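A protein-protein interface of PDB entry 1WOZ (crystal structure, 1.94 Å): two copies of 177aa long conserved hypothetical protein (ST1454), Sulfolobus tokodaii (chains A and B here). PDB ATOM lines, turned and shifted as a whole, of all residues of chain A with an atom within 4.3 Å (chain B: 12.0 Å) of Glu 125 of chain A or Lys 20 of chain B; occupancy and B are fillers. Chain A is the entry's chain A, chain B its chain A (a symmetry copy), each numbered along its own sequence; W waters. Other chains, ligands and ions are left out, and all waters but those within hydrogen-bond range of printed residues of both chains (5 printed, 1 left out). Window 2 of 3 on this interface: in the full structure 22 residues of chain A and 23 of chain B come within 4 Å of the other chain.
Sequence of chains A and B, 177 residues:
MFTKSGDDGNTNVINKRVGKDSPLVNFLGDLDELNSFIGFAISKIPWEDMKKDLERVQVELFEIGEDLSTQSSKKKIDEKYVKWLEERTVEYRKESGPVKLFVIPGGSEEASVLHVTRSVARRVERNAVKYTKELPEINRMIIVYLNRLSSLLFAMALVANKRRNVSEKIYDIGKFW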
ATOM      1  N   ALA A 121      -9.097  10.824 -35.096  1.00  0.00           N
ATOM      2  CA  ALA A 121      -9.797  12.003 -35.622  1.00  0.00           C
ATOM      3  C   ALA A 121     -10.482  12.736 -34.451  1.00  0.00           C
ATOM      4  O   ALA A 121     -10.478  13.971 -34.378  1.00  0.00           O
ATOM      5  CB  ALA A 121     -10.830  11.581 -36.666  1.00  0.00           C
ATOM      6  N   ARG A 122     -11.065  11.967 -33.531  1.00  0.00           N
ATOM      7  CA  ARG A 122     -11.726  12.553 -32.373  1.00  0.00           C
ATOM      8  C   ARG A 122     -10.715  13.244 -31.455  1.00  0.00           C
ATOM      9  O   ARG A 122     -11.023  14.300 -30.876  1.00  0.00           O
ATOM     10  CB  ARG A 122     -12.558  11.483 -31.632  1.00  0.00           C
ATOM     11  CG  ARG A 122     -13.870  11.188 -32.390  1.00  0.00           C
ATOM     12  CD  ARG A 122     -14.742  10.107 -31.733  1.00  0.00           C
ATOM     13  NE  ARG A 122     -15.179  10.409 -30.365  1.00  0.00           N
ATOM     14  CZ  ARG A 122     -16.300  11.050 -30.017  1.00  0.00           C
ATOM     15  NH1 ARG A 122     -17.149  11.497 -30.930  1.00  0.00           N
ATOM     16  NH2 ARG A 122     -16.600  11.207 -28.729  1.00  0.00           N
ATOM     17  N   ARG A 123      -9.489  12.713 -31.370  1.00  0.00           N
ATOM     18  CA  ARG A 123      -8.471  13.357 -30.543  1.00  0.00           C
ATOM     19  C   ARG A 123      -8.072  14.700 -31.187  1.00  0.00           C
ATOM     20  O   ARG A 123      -7.904  15.718 -30.485  1.00  0.00           O
ATOM     21  CB  ARG A 123      -7.241  12.443 -30.348  1.00  0.00           C
ATOM     22  CG  ARG A 123      -5.934  13.213 -30.000  1.00  0.00           C
ATOM     23  CD  ARG A 123      -4.912  12.360 -29.243  1.00  0.00           C
ATOM     24  NE  ARG A 123      -4.549  11.104 -29.912  1.00  0.00           N
ATOM     25  CZ  ARG A 123      -3.581  10.980 -30.815  1.00  0.00           C
ATOM     26  NH1 ARG A 123      -2.881  12.052 -31.171  1.00  0.00           N
ATOM     27  NH2 ARG A 123      -3.277   9.778 -31.318  1.00  0.00           N
ATOM     28  N   VAL A 124      -7.941  14.718 -32.513  1.00  0.00           N
ATOM     29  CA  VAL A 124      -7.605  15.954 -33.226  1.00  0.00           C
ATOM     30  C   VAL A 124      -8.756  16.959 -33.055  1.00  0.00           C
ATOM     31  O   VAL A 124      -8.519  18.156 -32.854  1.00  0.00           O
ATOM     32  CB  VAL A 124      -7.368  15.699 -34.747  1.00  0.00           C
ATOM     33  CG1 VAL A 124      -7.002  17.041 -35.468  1.00  0.00           C
ATOM     34  CG2 VAL A 124      -6.238  14.670 -34.927  1.00  0.00           C
ATOM     35  N   GLU A 125      -9.995  16.474 -33.115  1.00  0.00           N
ATOM     36  CA  GLU A 125     -11.164  17.355 -32.930  1.00  0.00           C
ATOM     37  C   GLU A 125     -11.127  18.033 -31.548  1.00  0.00           C
ATOM     38  O   GLU A 125     -11.314  19.257 -31.445  1.00  0.00           O
ATOM     39  CB  GLU A 125     -12.475  16.568 -33.074  1.00  0.00           C
ATOM     40  CG  GLU A 125     -13.713  17.458 -32.844  1.00  0.00           C
ATOM     41  CD  GLU A 125     -15.023  16.692 -32.812  1.00  0.00           C
ATOM     42  OE1 GLU A 125     -15.015  15.446 -32.962  1.00  0.00           O
ATOM     43  OE2 GLU A 125     -16.075  17.350 -32.639  1.00  0.00           O
ATOM     44  N   ARG A 126     -10.888  17.250 -30.489  1.00  0.00           N
ATOM     45  CA  ARG A 126     -10.793  17.821 -29.139  1.00  0.00           C
ATOM     46  C   ARG A 126      -9.640  18.816 -29.043  1.00  0.00           C
ATOM     47  O   ARG A 126      -9.796  19.896 -28.471  1.00  0.00           O
ATOM     48  CB  ARG A 126     -10.593  16.737 -28.065  1.00  0.00           C
ATOM     49  CG  ARG A 126     -11.799  15.814 -27.810  1.00  0.00           C
ATOM     50  CD  ARG A 126     -11.542  14.977 -26.545  1.00  0.00           C
ATOM     51  NE  ARG A 126     -10.249  14.278 -26.566  1.00  0.00           N
ATOM     52  CZ  ARG A 126      -9.994  13.151 -27.248  1.00  0.00           C
ATOM     53  NH1 ARG A 126     -10.933  12.567 -27.981  1.00  0.00           N
ATOM     54  NH2 ARG A 126      -8.791  12.594 -27.183  1.00  0.00           N
ATOM     55  N   ASN A 127      -8.471  18.456 -29.565  1.00  0.00           N
ATOM     56  CA  ASN A 127      -7.338  19.383 -29.536  1.00  0.00           C
ATOM     57  C   ASN A 127      -7.672  20.678 -30.300  1.00  0.00           C
ATOM     58  O   ASN A 127      -7.313  21.775 -29.866  1.00  0.00           O
ATOM     59  CB  ASN A 127      -6.083  18.731 -30.135  1.00  0.00           C
ATOM     60  CG  ASN A 127      -5.581  17.560 -29.304  1.00  0.00           C
ATOM     61  OD1 ASN A 127      -6.062  17.322 -28.195  1.00  0.00           O
ATOM     62  ND2 ASN A 127      -4.607  16.827 -29.835  1.00  0.00           N
ATOM     63  N   ALA A 128      -8.366  20.555 -31.432  1.00  0.00           N
ATOM     64  CA  ALA A 128      -8.739  21.731 -32.214  1.00  0.00           C
ATOM     65  C   ALA A 128      -9.543  22.719 -31.373  1.00  0.00           C
ATOM     66  O   ALA A 128      -9.327  23.934 -31.455  1.00  0.00           O
ATOM     67  CB  ALA A 128      -9.536  21.320 -33.454  1.00  0.00           C
ATOM     68  N   VAL A 129     -10.474  22.211 -30.571  1.00  0.00           N
ATOM     69  CA  VAL A 129     -11.265  23.072 -29.699  1.00  0.00           C
ATOM     70  C   VAL A 129     -10.322  23.801 -28.739  1.00  0.00           C
ATOM     71  O   VAL A 129     -10.471  24.996 -28.487  1.00  0.00           O
ATOM     72  CB  VAL A 129     -12.298  22.257 -28.893  1.00  0.00           C
ATOM     73  CG1 VAL A 129     -13.003  23.159 -27.882  1.00  0.00           C
ATOM     74  CG2 VAL A 129     -13.324  21.655 -29.842  1.00  0.00           C
ATOM     75  N   LEU A 146     -13.914  18.005 -38.976  1.00  0.00           N
ATOM     76  CA  LEU A 146     -13.323  16.945 -38.159  1.00  0.00           C
ATOM     77  C   LEU A 146     -14.397  16.113 -37.451  1.00  0.00           C
ATOM     78  O   LEU A 146     -14.276  14.888 -37.367  1.00  0.00           O
ATOM     79  CB  LEU A 146     -12.352  17.553 -37.144  1.00  0.00           C
ATOM     80  CG  LEU A 146     -11.037  18.081 -37.755  1.00  0.00           C
ATOM     81  CD1 LEU A 146     -10.257  18.798 -36.677  1.00  0.00           C
ATOM     82  CD2 LEU A 146     -10.195  16.916 -38.371  1.00  0.00           C
ATOM     83  N   ASN A 147     -15.441  16.779 -36.954  1.00  0.00           N
ATOM     84  CA  ASN A 147     -16.551  16.092 -36.282  1.00  0.00           C
ATOM     85  C   ASN A 147     -17.274  15.161 -37.258  1.00  0.00           C
ATOM     86  O   ASN A 147     -17.556  13.998 -36.925  1.00  0.00           O
ATOM     87  CB  ASN A 147     -17.508  17.134 -35.674  1.00  0.00           C
ATOM     88  CG  ASN A 147     -18.738  16.504 -34.984  1.00  0.00           C
ATOM     89  OD1 ASN A 147     -19.761  16.263 -35.620  1.00  0.00           O
ATOM     90  ND2 ASN A 147     -18.629  16.249 -33.684  1.00  0.00           N
ATOM     91  N   GLY B  19     -20.022  21.371 -23.701  1.00  0.00           N
ATOM     92  CA  GLY B  19     -18.624  21.869 -23.881  1.00  0.00           C
ATOM     93  C   GLY B  19     -17.595  20.753 -23.944  1.00  0.00           C
ATOM     94  O   GLY B  19     -17.540  19.890 -23.065  1.00  0.00           O
ATOM     95  N   LYS B  20     -16.775  20.777 -24.992  1.00  0.00           N
ATOM     96  CA  LYS B  20     -15.736  19.772 -25.194  1.00  0.00           C
ATOM     97  C   LYS B  20     -14.404  20.272 -24.637  1.00  0.00           C
ATOM     98  O   LYS B  20     -14.333  21.364 -24.054  1.00  0.00           O
ATOM     99  CB  LYS B  20     -15.606  19.470 -26.688  1.00  0.00           C
ATOM    100  CG  LYS B  20     -14.620  18.374 -27.050  1.00  0.00           C
ATOM    101  CD  LYS B  20     -14.877  17.892 -28.472  1.00  0.00           C
ATOM    102  CE  LYS B  20     -16.272  17.292 -28.595  1.00  0.00           C
ATOM    103  NZ  LYS B  20     -16.637  16.943 -29.995  1.00  0.00           N
ATOM    104  N   ASP B  21     -13.354  19.474 -24.822  1.00  0.00           N
ATOM    105  CA  ASP B  21     -12.016  19.804 -24.335  1.00  0.00           C
ATOM    106  C   ASP B  21     -11.963  19.700 -22.806  1.00  0.00           C
ATOM    107  O   ASP B  21     -10.922  19.924 -22.190  1.00  0.00           O
ATOM    108  CB  ASP B  21     -11.604  21.215 -24.772  1.00  0.00           C
ATOM    109  CG  ASP B  21     -10.112  21.471 -24.590  1.00  0.00           C
ATOM    110  OD1 ASP B  21      -9.694  22.645 -24.700  1.00  0.00           O
ATOM    111  OD2 ASP B  21      -9.356  20.500 -24.348  1.00  0.00           O
ATOM    112  N   SER B  22     -13.093  19.361 -22.198  1.00  0.00           N
ATOM    113  CA  SER B  22     -13.143  19.209 -20.754  1.00  0.00           C
ATOM    114  C   SER B  22     -12.349  17.961 -20.359  1.00  0.00           C
ATOM    115  O   SER B  22     -12.064  17.090 -21.196  1.00  0.00           O
ATOM    116  CB  SER B  22     -14.593  19.048 -20.292  1.00  0.00           C
ATOM    117  OG  SER B  22     -15.082  17.743 -20.577  1.00  0.00           O
ATOM    118  N   PRO B  23     -11.960  17.869 -19.082  1.00  0.00           N
ATOM    119  CA  PRO B  23     -11.205  16.708 -18.612  1.00  0.00           C
ATOM    120  C   PRO B  23     -12.013  15.427 -18.828  1.00  0.00           C
ATOM    121  O   PRO B  23     -11.465  14.415 -19.255  1.00  0.00           O
ATOM    122  CB  PRO B  23     -10.992  17.005 -17.132  1.00  0.00           C
ATOM    123  CG  PRO B  23     -10.937  18.495 -17.101  1.00  0.00           C
ATOM    124  CD  PRO B  23     -12.027  18.914 -18.043  1.00  0.00           C
ATOM    125  N   LEU B  24     -13.313  15.461 -18.529  1.00  0.00           N
ATOM    126  CA  LEU B  24     -14.117  14.260 -18.723  1.00  0.00           C
ATOM    127  C   LEU B  24     -14.157  13.814 -20.182  1.00  0.00           C
ATOM    128  O   LEU B  24     -13.937  12.640 -20.473  1.00  0.00           O
ATOM    129  CB  LEU B  24     -15.556  14.439 -18.226  1.00  0.00           C
ATOM    130  CG  LEU B  24     -16.454  13.210 -18.496  1.00  0.00           C
ATOM    131  CD1 LEU B  24     -15.914  11.992 -17.766  1.00  0.00           C
ATOM    132  CD2 LEU B  24     -17.890  13.491 -18.028  1.00  0.00           C
ATOM    133  N   VAL B  25     -14.437  14.748 -21.091  1.00  0.00           N
ATOM    134  CA  VAL B  25     -14.512  14.420 -22.514  1.00  0.00           C
ATOM    135  C   VAL B  25     -13.179  13.877 -23.028  1.00  0.00           C
ATOM    136  O   VAL B  25     -13.152  12.918 -23.805  1.00  0.00           O
ATOM    137  CB  VAL B  25     -14.939  15.646 -23.345  1.00  0.00           C
ATOM    138  CG1 VAL B  25     -14.905  15.306 -24.840  1.00  0.00           C
ATOM    139  CG2 VAL B  25     -16.360  16.058 -22.938  1.00  0.00           C
ATOM    140  N   ASN B  26     -12.080  14.487 -22.595  1.00  0.00           N
ATOM    141  CA  ASN B  26     -10.750  14.015 -22.986  1.00  0.00           C
ATOM    142  C   ASN B  26     -10.433  12.616 -22.418  1.00  0.00           C
ATOM    143  O   ASN B  26      -9.850  11.784 -23.108  1.00  0.00           O
ATOM    144  CB  ASN B  26      -9.688  15.024 -22.547  1.00  0.00           C
ATOM    145  CG  ASN B  26      -9.513  16.157 -23.552  1.00  0.00           C
ATOM    146  OD1 ASN B  26      -8.974  15.959 -24.646  1.00  0.00           O
ATOM    147  ND2 ASN B  26      -9.971  17.346 -23.192  1.00  0.00           N
ATOM    148  N   PHE B  27     -10.812  12.354 -21.168  1.00  0.00           N
ATOM    149  CA  PHE B  27     -10.578  11.048 -20.560  1.00  0.00           C
ATOM    150  C   PHE B  27     -11.365   9.993 -21.357  1.00  0.00           C
ATOM    151  O   PHE B  27     -10.830   8.935 -21.714  1.00  0.00           O
ATOM    152  CB  PHE B  27     -11.029  11.064 -19.083  1.00  0.00           C
ATOM    153  CG  PHE B  27     -10.413   9.980 -18.231  1.00  0.00           C
ATOM    154  CD1 PHE B  27     -10.449  10.079 -16.839  1.00  0.00           C
ATOM    155  CD2 PHE B  27      -9.809   8.856 -18.804  1.00  0.00           C
ATOM    156  CE1 PHE B  27      -9.899   9.078 -16.026  1.00  0.00           C
ATOM    157  CE2 PHE B  27      -9.248   7.849 -17.998  1.00  0.00           C
ATOM    158  CZ  PHE B  27      -9.298   7.965 -16.601  1.00  0.00           C
ATOM    159  N   LEU B  28     -12.638  10.271 -21.625  1.00  0.00           N
ATOM    160  CA  LEU B  28     -13.457   9.348 -22.411  1.00  0.00           C
ATOM    161  C   LEU B  28     -12.850   9.179 -23.814  1.00  0.00           C
ATOM    162  O   LEU B  28     -12.877   8.085 -24.371  1.00  0.00           O
ATOM    163  CB  LEU B  28     -14.898   9.863 -22.525  1.00  0.00           C
ATOM    164  CG  LEU B  28     -15.675   9.935 -21.200  1.00  0.00           C
ATOM    165  CD1 LEU B  28     -17.051  10.600 -21.452  1.00  0.00           C
ATOM    166  CD2 LEU B  28     -15.868   8.516 -20.640  1.00  0.00           C
ATOM    167  N   GLY B  29     -12.310  10.253 -24.378  1.00  0.00           N
ATOM    168  CA  GLY B  29     -11.688  10.152 -25.696  1.00  0.00           C
ATOM    169  C   GLY B  29     -10.460   9.245 -25.645  1.00  0.00           C
ATOM    170  O   GLY B  29     -10.236   8.423 -26.557  1.00  0.00           O
ATOM    171  N   ASP B  30      -9.653   9.382 -24.592  1.00  0.00           N
ATOM    172  CA  ASP B  30      -8.458   8.533 -24.449  1.00  0.00           C
ATOM    173  C   ASP B  30      -8.852   7.058 -24.284  1.00  0.00           C
ATOM    174  O   ASP B  30      -8.206   6.168 -24.841  1.00  0.00           O
ATOM    175  CB  ASP B  30      -7.606   8.974 -23.248  1.00  0.00           C
ATOM    176  CG  ASP B  30      -6.949  10.314 -23.468  1.00  0.00           C
ATOM    177  OD1 ASP B  30      -6.885  10.772 -24.628  1.00  0.00           O
ATOM    178  OD2 ASP B  30      -6.486  10.917 -22.483  1.00  0.00           O
ATOM    179  N   ASP B  32     -11.487   5.632 -25.496  1.00  0.00           N
ATOM    180  CA  ASP B  32     -11.919   5.157 -26.816  1.00  0.00           C
ATOM    181  C   ASP B  32     -10.695   4.848 -27.712  1.00  0.00           C
ATOM    182  O   ASP B  32     -10.664   3.832 -28.418  1.00  0.00           O
ATOM    183  CB  ASP B  32     -12.828   6.214 -27.471  1.00  0.00           C
ATOM    184  CG  ASP B  32     -13.251   5.839 -28.892  1.00  0.00           C
ATOM    185  OD1 ASP B  32     -13.596   4.671 -29.144  1.00  0.00           O
ATOM    186  OD2 ASP B  32     -13.252   6.729 -29.762  1.00  0.00           O
ATOM    187  N   GLU B  33      -9.693   5.723 -27.687  1.00  0.00           N
ATOM    188  CA  GLU B  33      -8.500   5.482 -28.495  1.00  0.00           C
ATOM    189  C   GLU B  33      -7.856   4.166 -28.043  1.00  0.00           C
ATOM    190  O   GLU B  33      -7.499   3.317 -28.857  1.00  0.00           O
ATOM    191  CB  GLU B  33      -7.514   6.661 -28.375  1.00  0.00           C
ATOM    192  CG  GLU B  33      -6.288   6.468 -29.284  1.00  0.00           C
ATOM    193  CD  GLU B  33      -5.301   7.636 -29.278  1.00  0.00           C
ATOM    194  OE1 GLU B  33      -5.585   8.680 -28.665  1.00  0.00           O
ATOM    195  OE2 GLU B  33      -4.230   7.510 -29.914  1.00  0.00           O
ATOM    196  N   ARG B 123      -0.168   5.788 -21.881  1.00  0.00           N
ATOM    197  CA  ARG B 123      -0.435   7.206 -22.115  1.00  0.00           C
ATOM    198  C   ARG B 123      -1.776   7.583 -21.454  1.00  0.00           C
ATOM    199  O   ARG B 123      -1.897   8.657 -20.829  1.00  0.00           O
ATOM    200  CB  ARG B 123      -0.443   7.537 -23.624  1.00  0.00           C
ATOM    201  CG  ARG B 123      -1.252   8.817 -23.983  1.00  0.00           C
ATOM    202  CD  ARG B 123      -0.796   9.475 -25.289  1.00  0.00           C
ATOM    203  NE  ARG B 123      -0.794   8.582 -26.454  1.00  0.00           N
ATOM    204  CZ  ARG B 123      -1.841   8.367 -27.244  1.00  0.00           C
ATOM    205  NH1 ARG B 123      -2.993   8.976 -26.980  1.00  0.00           N
ATOM    206  NH2 ARG B 123      -1.722   7.589 -28.326  1.00  0.00           N
ATOM    207  N   TYR B 131      -5.968  14.084 -15.194  1.00  0.00           N
ATOM    208  CA  TYR B 131      -7.386  14.427 -15.154  1.00  0.00           C
ATOM    209  C   TYR B 131      -7.929  14.401 -13.738  1.00  0.00           C
ATOM    210  O   TYR B 131      -8.859  15.150 -13.413  1.00  0.00           O
ATOM    211  CB  TYR B 131      -8.215  13.465 -15.998  1.00  0.00           C
ATOM    212  CG  TYR B 131      -7.831  13.425 -17.450  1.00  0.00           C
ATOM    213  CD1 TYR B 131      -7.569  14.601 -18.161  1.00  0.00           C
ATOM    214  CD2 TYR B 131      -7.765  12.211 -18.128  1.00  0.00           C
ATOM    215  CE1 TYR B 131      -7.244  14.558 -19.524  1.00  0.00           C
ATOM    216  CE2 TYR B 131      -7.450  12.158 -19.472  1.00  0.00           C
ATOM    217  CZ  TYR B 131      -7.188  13.323 -20.168  1.00  0.00           C
ATOM    218  OH  TYR B 131      -6.868  13.236 -21.503  1.00  0.00           O
ATOM    219  N   GLU B 134      -8.093  17.666 -12.060  1.00  0.00           N
ATOM    220  CA  GLU B 134      -9.202  18.535 -12.405  1.00  0.00           C
ATOM    221  C   GLU B 134     -10.539  17.945 -11.974  1.00  0.00           C
ATOM    222  O   GLU B 134     -11.523  18.664 -11.837  1.00  0.00           O
ATOM    223  CB  GLU B 134      -9.203  18.797 -13.903  1.00  0.00           C
ATOM    224  CG  GLU B 134      -7.975  19.564 -14.370  1.00  0.00           C
ATOM    225  CD  GLU B 134      -7.898  19.675 -15.879  1.00  0.00           C
ATOM    226  OE1 GLU B 134      -7.544  18.664 -16.531  1.00  0.00           O
ATOM    227  OE2 GLU B 134      -8.199  20.773 -16.407  1.00  0.00           O
ATOM    228  N   LEU B 135     -10.568  16.635 -11.753  1.00  0.00           N
ATOM    229  CA  LEU B 135     -11.789  15.947 -11.343  1.00  0.00           C
ATOM    230  C   LEU B 135     -11.469  14.980 -10.204  1.00  0.00           C
ATOM    231  O   LEU B 135     -11.446  13.769 -10.402  1.00  0.00           O
ATOM    232  CB  LEU B 135     -12.367  15.151 -12.517  1.00  0.00           C
ATOM    233  CG  LEU B 135     -12.591  15.868 -13.845  1.00  0.00           C
ATOM    234  CD1 LEU B 135     -12.980  14.845 -14.898  1.00  0.00           C
ATOM    235  CD2 LEU B 135     -13.677  16.925 -13.692  1.00  0.00           C
HETATM  236  O   HOH W   1     -14.903  12.223 -25.862  1.00  0.00           O
HETATM  237  O   HOH W   2     -10.314   9.861 -28.999  1.00  0.00           O
HETATM  238  O   HOH W   3      -7.459  17.863 -26.011  1.00  0.00           O
HETATM  239  O   HOH W   4      -6.905  13.619 -25.057  1.00  0.00           O
HETATM  240  O   HOH W   5     -12.875   9.390 -29.014  1.00  0.00           O
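Among the printed residues, merely in contact across the chains: Arg 126 of chain A with Gly 29 of chain B, Arg 126 of chain A with Lys 20 of chain B, Arg 126 of chain A with Val 25 of chain B, Val 129 of chain A with Asp 21 of chain B and Arg 123 of chain A with Arg 123 of chain B.
Arg 123 of chain B touches its own counterpart, Arg 123 of chain A.
The side-chain carboxylate (OD1) of Asp 30 of chain B lies within salt-bridge range of the guanidinium group (NH2) of Arg 126 of chain A, at 3.7 Å.
The side-chain amide oxygen (OD1) of Asn 26 of chain B lies within hydrogen-bond range of the guanidinium group (NE) of Arg 126 of chain A (2.9 Å).
The side-chain carboxylate (OE2) of Glu 125 of chain A is in salt-bridge range of the side-chain amino group (NZ) of Lys 20 of chain B (2.7 Å).
NH2 of Arg 123 of chain A lies within salt-bridge range of OE2 of Glu 33 of chain B (2.8 Å).
OG of Ser 22 of chain B sits at hydrogen-bond distance from N of Val 25 of chain B.
O of Arg 123 of chain A lies close to OD1 of Asn 127 of chain A (3.3 Å).
NH2 of Arg 123 of chain B lies within salt-bridge range of OE2 of Glu 33 of chain B (3.0 Å).
O of Ser 22 of chain B sits at hydrogen-bond distance from ND2 of Asn 26 of chain B, at 2.9 Å.
O of Arg 122 of chain A is in hydrogen-bond range of NH1 of Arg 126 of chain A (3.4 Å).
O of Asp 21 of chain B is in hydrogen-bond range of ND2 of Asn 26 of chain B (2.9 Å).
Water W3 lies within hydrogen-bond range of the side-chain amide oxygen of Asn 127 of chain A and the side-chain amide oxygen of Asn 26 of chain B.
Water W5 bridges the side-chain carboxylate of Asp 32 of chain B (2.8 Å) and the guanidinium group of Arg 122 of chain A (2.9 Å).
Water W1 bridges O of Val 25 of chain B (2.8 Å) and NH2 of Arg 122 of chain A (3.5 Å).
Water W2 lies within hydrogen-bond range of O of Gly 29 of chain B (2.8 Å) and NH1 of Arg 126 of chain A (3.0 Å).
Water W4 lies within hydrogen-bond range of OD1 of Asp 30 of chain B, NH2 of Arg 126 of chain A and OD1 of Asn 26 of chain B.
Of the 11 printed residues of chain A, 4 touch a printed residue of chain B.
Hydrophobic or aromatic side chains of chain A within 4 Å of the printed part of chain B: Val 129.
Hydrophobic or aromatic side chains of chain B that line the printed part of chain A: Val 25.
Among the printed residues, 9 pairs touch across the chains.
Among the printed residues, Asp or Glu carboxylates within 4 Å of a Lys or Arg side-chain nitrogen of the other chain: Arg 123 of chain A with Glu 33 of chain B (2.8 Å), Glu 125 of chain A with Lys 20 of chain B (2.7 Å) and Arg 126 of chain A with Asp 30 of chain B (3.7 Å).
Printed residues of chain B within 4 Å of Arg 123 of chain A: Glu 33 and Arg 123.
No residue of chain B comes within 4 Å of Val 124 of chain A.
Glu 125 of chain A touches one residue of chain B.
Val 129 of chain A touches just one residue of chain B: Asp 21 (3.9 Å).
No residue of chain B comes within 4 Å of Leu 146 of chain A.
Gly 19 of chain B touches none of the printed residues of chain A.
Lys 20 of chain B touches just these residues of chain A: Glu 125 and Arg 126.
Of the printed residues of chain A, Val 25 of chain B touches Arg 126 (3.8 Å).
Printed residues of chain A within 4 Å of Asn 26 of chain B: Arg 126 (2.9 Å).
Of the printed residues of chain A, Asp 30 of chain B touches Arg 126.
Tyr 131 of chain B touches none of the printed residues of chain A.
The nearest residue of chain A that does not touch Lys 20 of chain B is Asn 147 of chain A (4.2 Å).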
